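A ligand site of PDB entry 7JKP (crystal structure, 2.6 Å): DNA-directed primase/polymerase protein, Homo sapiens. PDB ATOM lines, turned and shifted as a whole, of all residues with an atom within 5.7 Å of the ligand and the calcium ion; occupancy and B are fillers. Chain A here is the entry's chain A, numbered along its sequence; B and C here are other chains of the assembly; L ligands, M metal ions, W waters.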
ATOM      1  N   GLY A  74      -9.943  -0.174  32.606  1.00  0.00           N
ATOM      2  CA  GLY A  74     -11.385  -0.181  32.541  1.00  0.00           C
ATOM      3  C   GLY A  74     -12.079  -0.549  33.838  1.00  0.00           C
ATOM      4  O   GLY A  74     -13.297  -0.775  33.814  1.00  0.00           O
ATOM      5  N   ARG A  76     -14.323  -0.614  36.744  1.00  0.00           N
ATOM      6  CA  ARG A  76     -15.567   0.131  36.826  1.00  0.00           C
ATOM      7  C   ARG A  76     -16.278  -0.161  38.144  1.00  0.00           C
ATOM      8  O   ARG A  76     -16.224  -1.277  38.653  1.00  0.00           O
ATOM      9  CB  ARG A  76     -16.493  -0.224  35.658  1.00  0.00           C
ATOM     10  CG  ARG A  76     -16.175   0.511  34.368  1.00  0.00           C
ATOM     11  CD  ARG A  76     -16.699  -0.240  33.165  1.00  0.00           C
ATOM     12  NE  ARG A  76     -16.795   0.588  31.962  1.00  0.00           N
ATOM     13  CZ  ARG A  76     -15.745   0.989  31.239  1.00  0.00           C
ATOM     14  NH1 ARG A  76     -14.521   0.650  31.598  1.00  0.00           N
ATOM     15  NH2 ARG A  76     -15.933   1.732  30.161  1.00  0.00           N
ATOM     16  N   TYR A 100     -21.010   5.800  32.214  1.00  0.00           N
ATOM     17  CA  TYR A 100     -21.478   4.965  31.113  1.00  0.00           C
ATOM     18  C   TYR A 100     -22.859   4.415  31.445  1.00  0.00           C
ATOM     19  O   TYR A 100     -23.172   4.138  32.616  1.00  0.00           O
ATOM     20  CB  TYR A 100     -20.522   3.812  30.841  1.00  0.00           C
ATOM     21  CG  TYR A 100     -19.146   4.253  30.408  1.00  0.00           C
ATOM     22  CD1 TYR A 100     -18.179   4.612  31.346  1.00  0.00           C
ATOM     23  CD2 TYR A 100     -18.793   4.316  29.064  1.00  0.00           C
ATOM     24  CE1 TYR A 100     -16.919   5.020  30.955  1.00  0.00           C
ATOM     25  CE2 TYR A 100     -17.542   4.720  28.664  1.00  0.00           C
ATOM     26  CZ  TYR A 100     -16.611   5.074  29.611  1.00  0.00           C
ATOM     27  OH  TYR A 100     -15.357   5.479  29.227  1.00  0.00           O
ATOM     28  N   ASP A 114     -22.391   2.778  17.141  1.00  0.00           N
ATOM     29  CA  ASP A 114     -21.071   3.294  17.488  1.00  0.00           C
ATOM     30  C   ASP A 114     -20.297   3.427  16.189  1.00  0.00           C
ATOM     31  O   ASP A 114     -19.941   2.426  15.552  1.00  0.00           O
ATOM     32  CB  ASP A 114     -20.349   2.367  18.473  1.00  0.00           C
ATOM     33  CG  ASP A 114     -18.955   2.881  18.827  1.00  0.00           C
ATOM     34  OD1 ASP A 114     -18.651   4.047  18.504  1.00  0.00           O
ATOM     35  OD2 ASP A 114     -18.161   2.118  19.416  1.00  0.00           O
ATOM     36  N   LEU A 115     -20.032   4.669  15.790  1.00  0.00           N
ATOM     37  CA  LEU A 115     -19.349   4.967  14.543  1.00  0.00           C
ATOM     38  C   LEU A 115     -17.974   5.547  14.847  1.00  0.00           C
ATOM     39  O   LEU A 115     -17.852   6.500  15.635  1.00  0.00           O
ATOM     40  CB  LEU A 115     -20.161   5.952  13.698  1.00  0.00           C
ATOM     41  CG  LEU A 115     -21.605   5.520  13.419  1.00  0.00           C
ATOM     42  CD1 LEU A 115     -22.306   6.546  12.545  1.00  0.00           C
ATOM     43  CD2 LEU A 115     -21.665   4.141  12.761  1.00  0.00           C
ATOM     44  N   GLU A 116     -16.941   4.966  14.244  1.00  0.00           N
ATOM     45  CA  GLU A 116     -15.573   5.408  14.504  1.00  0.00           C
ATOM     46  C   GLU A 116     -14.600   4.873  13.469  1.00  0.00           C
ATOM     47  O   GLU A 116     -14.611   3.675  13.150  1.00  0.00           O
ATOM     48  CB  GLU A 116     -15.137   4.978  15.910  1.00  0.00           C
ATOM     49  CG  GLU A 116     -15.276   3.479  16.168  1.00  0.00           C
ATOM     50  CD  GLU A 116     -14.550   3.040  17.426  1.00  0.00           C
ATOM     51  OE1 GLU A 116     -13.933   1.948  17.410  1.00  0.00           O
ATOM     52  OE2 GLU A 116     -14.591   3.786  18.432  1.00  0.00           O
ATOM     53  N   SER A 160     -17.896  12.761  19.595  1.00  0.00           N
ATOM     54  CA  SER A 160     -16.797  12.649  20.549  1.00  0.00           C
ATOM     55  C   SER A 160     -15.469  12.564  19.811  1.00  0.00           C
ATOM     56  O   SER A 160     -14.528  11.920  20.289  1.00  0.00           O
ATOM     57  CB  SER A 160     -16.979  11.430  21.456  1.00  0.00           C
ATOM     58  OG  SER A 160     -15.950  11.353  22.429  1.00  0.00           O
ATOM     59  N   LYS A 165      -9.597  10.698  15.368  1.00  0.00           N
ATOM     60  CA  LYS A 165     -10.687   9.730  15.412  1.00  0.00           C
ATOM     61  C   LYS A 165     -12.016  10.439  15.189  1.00  0.00           C
ATOM     62  O   LYS A 165     -12.411  11.278  16.001  1.00  0.00           O
ATOM     63  CB  LYS A 165     -10.709   8.982  16.753  1.00  0.00           C
ATOM     64  CG  LYS A 165     -11.694   7.834  16.791  1.00  0.00           C
ATOM     65  CD  LYS A 165     -11.546   7.011  18.065  1.00  0.00           C
ATOM     66  CE  LYS A 165     -12.484   5.812  18.061  1.00  0.00           C
ATOM     67  NZ  LYS A 165     -12.326   4.962  19.270  1.00  0.00           N
ATOM     68  N   SER A 167     -15.418  10.090  15.771  1.00  0.00           N
ATOM     69  CA  SER A 167     -16.236   9.264  16.654  1.00  0.00           C
ATOM     70  C   SER A 167     -17.623   9.867  16.778  1.00  0.00           C
ATOM     71  O   SER A 167     -17.758  11.057  17.107  1.00  0.00           O
ATOM     72  CB  SER A 167     -15.573   9.135  18.027  1.00  0.00           C
ATOM     73  OG  SER A 167     -16.338   8.335  18.895  1.00  0.00           O
ATOM     74  N   HIS A 169     -21.897   8.878  17.987  1.00  0.00           N
ATOM     75  CA  HIS A 169     -22.893   7.998  18.566  1.00  0.00           C
ATOM     76  C   HIS A 169     -24.269   8.407  18.051  1.00  0.00           C
ATOM     77  O   HIS A 169     -24.653   9.578  18.160  1.00  0.00           O
ATOM     78  CB  HIS A 169     -22.882   8.055  20.094  1.00  0.00           C
ATOM     79  CG  HIS A 169     -21.816   7.211  20.723  1.00  0.00           C
ATOM     80  ND1 HIS A 169     -21.789   6.934  22.078  1.00  0.00           N
ATOM     81  CD2 HIS A 169     -20.741   6.579  20.193  1.00  0.00           C
ATOM     82  CE1 HIS A 169     -20.737   6.177  22.351  1.00  0.00           C
ATOM     83  NE2 HIS A 169     -20.087   5.944  21.218  1.00  0.00           N
ATOM     84  N   ASP A 280     -19.300  -0.100  14.244  1.00  0.00           N
ATOM     85  CA  ASP A 280     -18.730  -0.976  15.265  1.00  0.00           C
ATOM     86  C   ASP A 280     -19.805  -1.955  15.699  1.00  0.00           C
ATOM     87  O   ASP A 280     -20.726  -1.601  16.448  1.00  0.00           O
ATOM     88  CB  ASP A 280     -18.212  -0.152  16.444  1.00  0.00           C
ATOM     89  CG  ASP A 280     -17.602  -1.004  17.531  1.00  0.00           C
ATOM     90  OD1 ASP A 280     -17.565  -2.243  17.372  1.00  0.00           O
ATOM     91  OD2 ASP A 280     -17.145  -0.438  18.549  1.00  0.00           O
ATOM     92  N   VAL A 283     -20.606  -3.620  19.895  1.00  0.00           N
ATOM     93  CA  VAL A 283     -21.262  -2.946  21.015  1.00  0.00           C
ATOM     94  C   VAL A 283     -22.596  -3.584  21.374  1.00  0.00           C
ATOM     95  O   VAL A 283     -23.278  -3.081  22.280  1.00  0.00           O
ATOM     96  CB  VAL A 283     -21.464  -1.451  20.717  1.00  0.00           C
ATOM     97  CG1 VAL A 283     -20.118  -0.737  20.586  1.00  0.00           C
ATOM     98  CG2 VAL A 283     -22.307  -1.250  19.469  1.00  0.00           C
ATOM     99  N   ARG A 288     -23.855  -4.174  27.992  1.00  0.00           N
ATOM    100  CA  ARG A 288     -22.881  -3.287  27.370  1.00  0.00           C
ATOM    101  C   ARG A 288     -22.880  -1.922  28.043  1.00  0.00           C
ATOM    102  O   ARG A 288     -23.939  -1.384  28.389  1.00  0.00           O
ATOM    103  CB  ARG A 288     -23.175  -3.139  25.881  1.00  0.00           C
ATOM    104  CG  ARG A 288     -22.358  -2.054  25.174  1.00  0.00           C
ATOM    105  CD  ARG A 288     -20.859  -2.351  25.227  1.00  0.00           C
ATOM    106  NE  ARG A 288     -20.518  -3.599  24.534  1.00  0.00           N
ATOM    107  CZ  ARG A 288     -19.283  -4.048  24.383  1.00  0.00           C
ATOM    108  NH1 ARG A 288     -18.257  -3.373  24.865  1.00  0.00           N
ATOM    109  NH2 ARG A 288     -19.066  -5.190  23.738  1.00  0.00           N
ATOM    110  N   ASN A 289     -21.688  -1.372  28.243  1.00  0.00           N
ATOM    111  CA  ASN A 289     -21.542  -0.002  28.693  1.00  0.00           C
ATOM    112  C   ASN A 289     -21.490   0.916  27.476  1.00  0.00           C
ATOM    113  O   ASN A 289     -20.942   0.550  26.434  1.00  0.00           O
ATOM    114  CB  ASN A 289     -20.267   0.166  29.525  1.00  0.00           C
ATOM    115  CG  ASN A 289     -20.356  -0.507  30.898  1.00  0.00           C
ATOM    116  OD1 ASN A 289     -19.478  -0.303  31.735  1.00  0.00           O
ATOM    117  ND2 ASN A 289     -21.397  -1.304  31.122  1.00  0.00           N
ATOM    118  N   PHE A 290     -22.079   2.104  27.607  1.00  0.00           N
ATOM    119  CA  PHE A 290     -22.150   3.054  26.511  1.00  0.00           C
ATOM    120  C   PHE A 290     -22.003   4.456  27.076  1.00  0.00           C
ATOM    121  O   PHE A 290     -22.830   4.890  27.885  1.00  0.00           O
ATOM    122  CB  PHE A 290     -23.468   2.901  25.741  1.00  0.00           C
ATOM    123  CG  PHE A 290     -23.374   3.297  24.293  1.00  0.00           C
ATOM    124  CD1 PHE A 290     -22.438   2.707  23.451  1.00  0.00           C
ATOM    125  CD2 PHE A 290     -24.239   4.238  23.762  1.00  0.00           C
ATOM    126  CE1 PHE A 290     -22.362   3.068  22.124  1.00  0.00           C
ATOM    127  CE2 PHE A 290     -24.167   4.598  22.418  1.00  0.00           C
ATOM    128  CZ  PHE A 290     -23.223   4.011  21.610  1.00  0.00           C
ATOM    129  N   ARG A 291     -20.947   5.158  26.668  1.00  0.00           N
ATOM    130  CA  ARG A 291     -20.605   6.443  27.253  1.00  0.00           C
ATOM    131  C   ARG A 291     -21.799   7.392  27.208  1.00  0.00           C
ATOM    132  O   ARG A 291     -22.436   7.566  26.159  1.00  0.00           O
ATOM    133  CB  ARG A 291     -19.407   7.049  26.523  1.00  0.00           C
ATOM    134  CG  ARG A 291     -18.849   8.316  27.174  1.00  0.00           C
ATOM    135  CD  ARG A 291     -17.339   8.419  27.018  1.00  0.00           C
ATOM    136  NE  ARG A 291     -16.903   8.263  25.641  1.00  0.00           N
ATOM    137  CZ  ARG A 291     -16.704   9.256  24.776  1.00  0.00           C
ATOM    138  NH1 ARG A 291     -16.906  10.520  25.137  1.00  0.00           N
ATOM    139  NH2 ARG A 291     -16.309   8.989  23.545  1.00  0.00           N
ATOM    140  N   LYS A 297     -13.959   9.505  28.380  1.00  0.00           N
ATOM    141  CA  LYS A 297     -13.249   8.403  29.016  1.00  0.00           C
ATOM    142  C   LYS A 297     -12.284   8.936  30.068  1.00  0.00           C
ATOM    143  O   LYS A 297     -11.874  10.101  30.042  1.00  0.00           O
ATOM    144  CB  LYS A 297     -12.488   7.588  27.969  1.00  0.00           C
ATOM    145  CG  LYS A 297     -13.361   7.020  26.864  1.00  0.00           C
ATOM    146  CD  LYS A 297     -12.659   5.895  26.129  1.00  0.00           C
ATOM    147  CE  LYS A 297     -13.464   5.403  24.929  1.00  0.00           C
ATOM    148  NZ  LYS A 297     -12.740   4.338  24.177  1.00  0.00           N
ATOM    149  N   LEU A 304     -19.028  13.499  24.908  1.00  0.00           N
ATOM    150  CA  LEU A 304     -20.070  13.405  23.890  1.00  0.00           C
ATOM    151  C   LEU A 304     -20.958  14.640  23.924  1.00  0.00           C
ATOM    152  O   LEU A 304     -21.417  15.061  24.988  1.00  0.00           O
ATOM    153  CB  LEU A 304     -20.912  12.146  24.120  1.00  0.00           C
ATOM    154  CG  LEU A 304     -20.287  10.839  23.641  1.00  0.00           C
ATOM    155  CD1 LEU A 304     -20.907   9.653  24.361  1.00  0.00           C
ATOM    156  CD2 LEU A 304     -20.464  10.691  22.137  1.00  0.00           C
ATOM    157  P    DG B  13     -11.504  -2.274  19.108  1.00  0.00           P
ATOM    158  OP1  DG B  13     -11.874  -2.356  17.678  1.00  0.00           O
ATOM    159  OP2  DG B  13     -10.577  -1.222  19.576  1.00  0.00           O
ATOM    160  O5'  DG B  13     -12.835  -2.166  19.982  1.00  0.00           O
ATOM    161  C5'  DG B  13     -13.895  -3.097  19.783  1.00  0.00           C
ATOM    162  C4'  DG B  13     -14.907  -3.019  20.908  1.00  0.00           C
ATOM    163  O4'  DG B  13     -14.370  -3.664  22.086  1.00  0.00           O
ATOM    164  C3'  DG B  13     -15.275  -1.596  21.351  1.00  0.00           C
ATOM    165  O3'  DG B  13     -16.614  -1.292  20.969  1.00  0.00           O
ATOM    166  C2'  DG B  13     -15.077  -1.591  22.871  1.00  0.00           C
ATOM    167  C1'  DG B  13     -14.917  -3.055  23.223  1.00  0.00           C
ATOM    168  N9   DG B  13     -14.027  -3.301  24.352  1.00  0.00           N
ATOM    169  C8   DG B  13     -12.700  -2.974  24.454  1.00  0.00           C
ATOM    170  N7   DG B  13     -12.158  -3.316  25.589  1.00  0.00           N
ATOM    171  C5   DG B  13     -13.197  -3.909  26.293  1.00  0.00           C
ATOM    172  C6   DG B  13     -13.219  -4.492  27.588  1.00  0.00           C
ATOM    173  O6   DG B  13     -12.285  -4.584  28.400  1.00  0.00           O
ATOM    174  N1   DG B  13     -14.480  -4.984  27.916  1.00  0.00           N
ATOM    175  C2   DG B  13     -15.578  -4.930  27.092  1.00  0.00           C
ATOM    176  N2   DG B  13     -16.710  -5.462  27.579  1.00  0.00           N
ATOM    177  N3   DG B  13     -15.570  -4.396  25.877  1.00  0.00           N
ATOM    178  C4   DG B  13     -14.355  -3.914  25.548  1.00  0.00           C
ATOM    179  P   8OG C   3     -12.100  -5.722  39.042  1.00  0.00           P
ATOM    180  OP1 8OG C   3     -11.467  -7.012  38.548  1.00  0.00           O
ATOM    181  OP2 8OG C   3     -11.081  -4.649  39.195  1.00  0.00           O
ATOM    182  O5' 8OG C   3     -13.308  -5.252  38.048  1.00  0.00           O
ATOM    183  C5' 8OG C   3     -14.101  -4.187  38.440  1.00  0.00           C
ATOM    184  C4' 8OG C   3     -15.420  -4.227  37.701  1.00  0.00           C
ATOM    185  O4' 8OG C   3     -15.352  -3.512  36.638  1.00  0.00           O
ATOM    186  C3' 8OG C   3     -15.784  -5.774  37.248  1.00  0.00           C
ATOM    187  O3' 8OG C   3     -17.188  -6.068  37.661  1.00  0.00           O
ATOM    188  C2' 8OG C   3     -15.652  -5.850  36.029  1.00  0.00           C
ATOM    189  C1' 8OG C   3     -15.784  -4.379  35.490  1.00  0.00           C
ATOM    190  N9  8OG C   3     -14.984  -4.149  34.438  1.00  0.00           N
ATOM    191  C8  8OG C   3     -15.410  -3.814  33.026  1.00  0.00           C
ATOM    192  N7  8OG C   3     -14.145  -3.622  32.221  1.00  0.00           N
ATOM    193  C5  8OG C   3     -13.046  -3.840  33.132  1.00  0.00           C
ATOM    194  C6  8OG C   3     -11.539  -3.784  32.869  1.00  0.00           C
ATOM    195  O6  8OG C   3     -11.115  -3.519  31.745  1.00  0.00           O
ATOM    196  N1  8OG C   3     -10.608  -4.046  33.960  1.00  0.00           N
ATOM    197  C2  8OG C   3     -11.119  -4.354  35.305  1.00  0.00           C
ATOM    198  N2  8OG C   3     -10.177  -4.618  36.417  1.00  0.00           N
ATOM    199  N3  8OG C   3     -12.572  -4.413  35.545  1.00  0.00           N
ATOM    200  C4  8OG C   3     -13.535  -4.141  34.430  1.00  0.00           C
ATOM    201  O8  8OG C   3     -16.487  -3.715  32.640  1.00  0.00           O
ATOM    202  P    DC C   4     -17.724  -7.572  37.713  1.00  0.00           P
ATOM    203  OP1  DC C   4     -18.911  -7.607  38.598  1.00  0.00           O
ATOM    204  OP2  DC C   4     -16.570  -8.457  37.994  1.00  0.00           O
ATOM    205  O5'  DC C   4     -18.205  -7.853  36.215  1.00  0.00           O
ATOM    206  C5'  DC C   4     -19.182  -7.014  35.631  1.00  0.00           C
ATOM    207  C4'  DC C   4     -19.132  -7.071  34.113  1.00  0.00           C
ATOM    208  O4'  DC C   4     -17.840  -6.608  33.644  1.00  0.00           O
ATOM    209  C3'  DC C   4     -19.301  -8.467  33.505  1.00  0.00           C
ATOM    210  O3'  DC C   4     -20.609  -8.590  32.962  1.00  0.00           O
ATOM    211  C2'  DC C   4     -18.207  -8.544  32.421  1.00  0.00           C
ATOM    212  C1'  DC C   4     -17.668  -7.130  32.359  1.00  0.00           C
ATOM    213  N1   DC C   4     -16.219  -7.022  31.984  1.00  0.00           N
ATOM    214  C2   DC C   4     -15.863  -6.626  30.696  1.00  0.00           C
ATOM    215  O2   DC C   4     -16.755  -6.377  29.871  1.00  0.00           O
ATOM    216  N3   DC C   4     -14.559  -6.525  30.373  1.00  0.00           N
ATOM    217  C4   DC C   4     -13.617  -6.800  31.284  1.00  0.00           C
ATOM    218  N4   DC C   4     -12.333  -6.685  30.923  1.00  0.00           N
ATOM    219  C5   DC C   4     -13.960  -7.206  32.606  1.00  0.00           C
ATOM    220  C6   DC C   4     -15.260  -7.298  32.909  1.00  0.00           C
HETATM  221  P1  LIG L   1     -14.637   6.403  21.356  1.00  0.00           P
HETATM  222  O1  LIG L   1     -13.178   6.166  21.763  1.00  0.00           O
HETATM  223  O2  LIG L   1     -15.106   5.241  20.478  1.00  0.00           O
HETATM  224  O3  LIG L   1     -14.752   7.667  20.602  1.00  0.00           O
HETATM  225  P2  LIG L   1     -16.743   5.367  22.915  1.00  0.00           P
HETATM  226  O4  LIG L   1     -17.815   5.947  23.855  1.00  0.00           O
HETATM  227  O5  LIG L   1     -17.348   5.043  21.569  1.00  0.00           O
HETATM  228  O6  LIG L   1     -15.570   6.445  22.680  1.00  0.00           O
HETATM  229  P3  LIG L   1     -15.482   2.730  22.725  1.00  0.00           P
HETATM  230  O7  LIG L   1     -14.053   2.504  23.150  1.00  0.00           O
HETATM  231  O8  LIG L   1     -15.524   3.098  21.252  1.00  0.00           O
HETATM  232  O9  LIG L   1     -16.139   3.995  23.614  1.00  0.00           O
HETATM  233  O10 LIG L   1     -16.355   1.347  22.987  1.00  0.00           O
HETATM  234  C1  LIG L   1     -17.790   1.412  22.960  1.00  0.00           C
HETATM  235  C2  LIG L   1     -18.346   1.004  24.319  1.00  0.00           C
HETATM  236  O11 LIG L   1     -17.847  -0.118  24.673  1.00  0.00           O
HETATM  237  C3  LIG L   1     -17.878   2.103  25.495  1.00  0.00           C
HETATM  238  O12 LIG L   1     -18.771   3.283  25.483  1.00  0.00           O
HETATM  239  C4  LIG L   1     -17.980   1.487  26.544  1.00  0.00           C
HETATM  240  C5  LIG L   1     -17.612  -0.010  26.174  1.00  0.00           C
HETATM  241  N1  LIG L   1     -16.355  -0.217  26.464  1.00  0.00           N
HETATM  242  C6  LIG L   1     -15.282   0.163  25.768  1.00  0.00           C
HETATM  243  N2  LIG L   1     -14.197  -0.252  26.440  1.00  0.00           N
HETATM  244  C7  LIG L   1     -14.604  -0.880  27.555  1.00  0.00           C
HETATM  245  C8  LIG L   1     -13.917  -1.487  28.576  1.00  0.00           C
HETATM  246  N3  LIG L   1     -12.574  -1.737  28.963  1.00  0.00           N
HETATM  247  N4  LIG L   1     -14.578  -2.051  29.582  1.00  0.00           N
HETATM  248  C9  LIG L   1     -15.925  -2.037  29.599  1.00  0.00           C
HETATM  249  N5  LIG L   1     -16.597  -1.439  28.588  1.00  0.00           N
HETATM  250  C10 LIG L   1     -15.935  -0.860  27.574  1.00  0.00           C
HETATM  251 CA    CA M   1     -16.566   3.981  19.625  1.00  0.00          CA
HETATM  252  O   HOH W   1     -17.292   6.007  18.799  1.00  0.00           O
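O2 of the ligand binds the calcium ion (2.1 Å). O8 of the ligand is bound to the calcium ion (2.1 Å). Water W1 is bound to the calcium ion (2.3 Å). The calcium ion is bound by the side-chain carboxylate (OE2) of Glu 116 (2.3 Å). An oxygen (O5) of the ligand binds the calcium ion (2.3 Å). OD1 of Asp 114 binds the calcium ion (2.4 Å). OD2 of Asp 114 is bound to the calcium ion, 2.5 Å away. The calcium ion has seven donor atoms within binding distance.
A nitrogen (N3) of the ligand is in hydrogen-bond range of O6 of DG 13 of chain B. O4 of the ligand sits close to NE2 of His 169 (3.5 Å). NE of Arg 291 is in salt-bridge range of O4 of the ligand, at 3.1 Å. An oxygen (O11) of the ligand is in hydrogen-bond range of the guanidinium group (NH1) of Arg 288 (3.3 Å). O7 of the ligand lies within salt-bridge range of NZ of Lys 297. N of Arg 291 sits at hydrogen-bond distance from O12 of the ligand (3.1 Å). O1 of the ligand lies within salt-bridge range of NZ of Lys 165, 2.9 Å away. OG of Ser 167 is in hydrogen-bond range of O3 of the ligand (2.4 Å). The guanidinium group (NH1) of Arg 76 is in hydrogen-bond range of a nitrogen (N4) of the ligand, at 3.4 Å.
N7 of 8OG 3 of chain C sits close to a nitrogen (N4) of the ligand (3.1 Å). Residues that only touch the ligand: Tyr 100, Val 283, Asn 289 and Phe 290. Hydrophobic or aromatic side chains within 4 Å of the ligand: Tyr 100, His 169 and Val 283. Within 4 Å of the ligand: Arg 76, Tyr 100, Asp 114, Glu 116, Lys 165, Ser 167, His 169, Val 283, Arg 288, Asn 289, Phe 290, Arg 291, Lys 297, DG 13 of chain B and 8OG 3 of chain C. The nearest printed residue that does not touch the ligand is Gly 74 (4.1 Å).
Two residues have an atom within 4 Å of the calcium ion: Asp 114 and Glu 116. Along chain A the residues within 4 Å of the calcium ion span positions 114 to 116. The nearest printed residue that does not touch the calcium ion is His 169 (4.3 Å).
Water W1 bridges the side-chain hydroxyl (OG) of Ser 167 and the backbone carbonyl oxygen (O) of Leu 115.
O3' of DG 13 of chain B lies close to the side-chain carboxylate (OD2) of Asp 280 (2.6 Å). N2 of DG 13 of chain B lies close to O2 of DC 4 of chain C (2.5 Å). NH1 of Arg 76 lies within hydrogen-bond range of O of Gly 74 (2.9 Å). The guanidinium group (NH1) of Arg 288 lies within hydrogen-bond range of N3 of DG 13 of chain B (3.0 Å). The backbone NH of Asp 280 sits at hydrogen-bond distance from the backbone carbonyl oxygen of Asp 114, at 2.9 Å. O4' of 8OG 3 of chain C sits at hydrogen-bond distance from N of Arg 76, at 3.1 Å. OD1 of Asn 289 is in hydrogen-bond range of NE of Arg 76, at 2.8 Å. The backbone carbonyl oxygen of Ser 167 sits at hydrogen-bond distance from the backbone NH of Ser 160.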
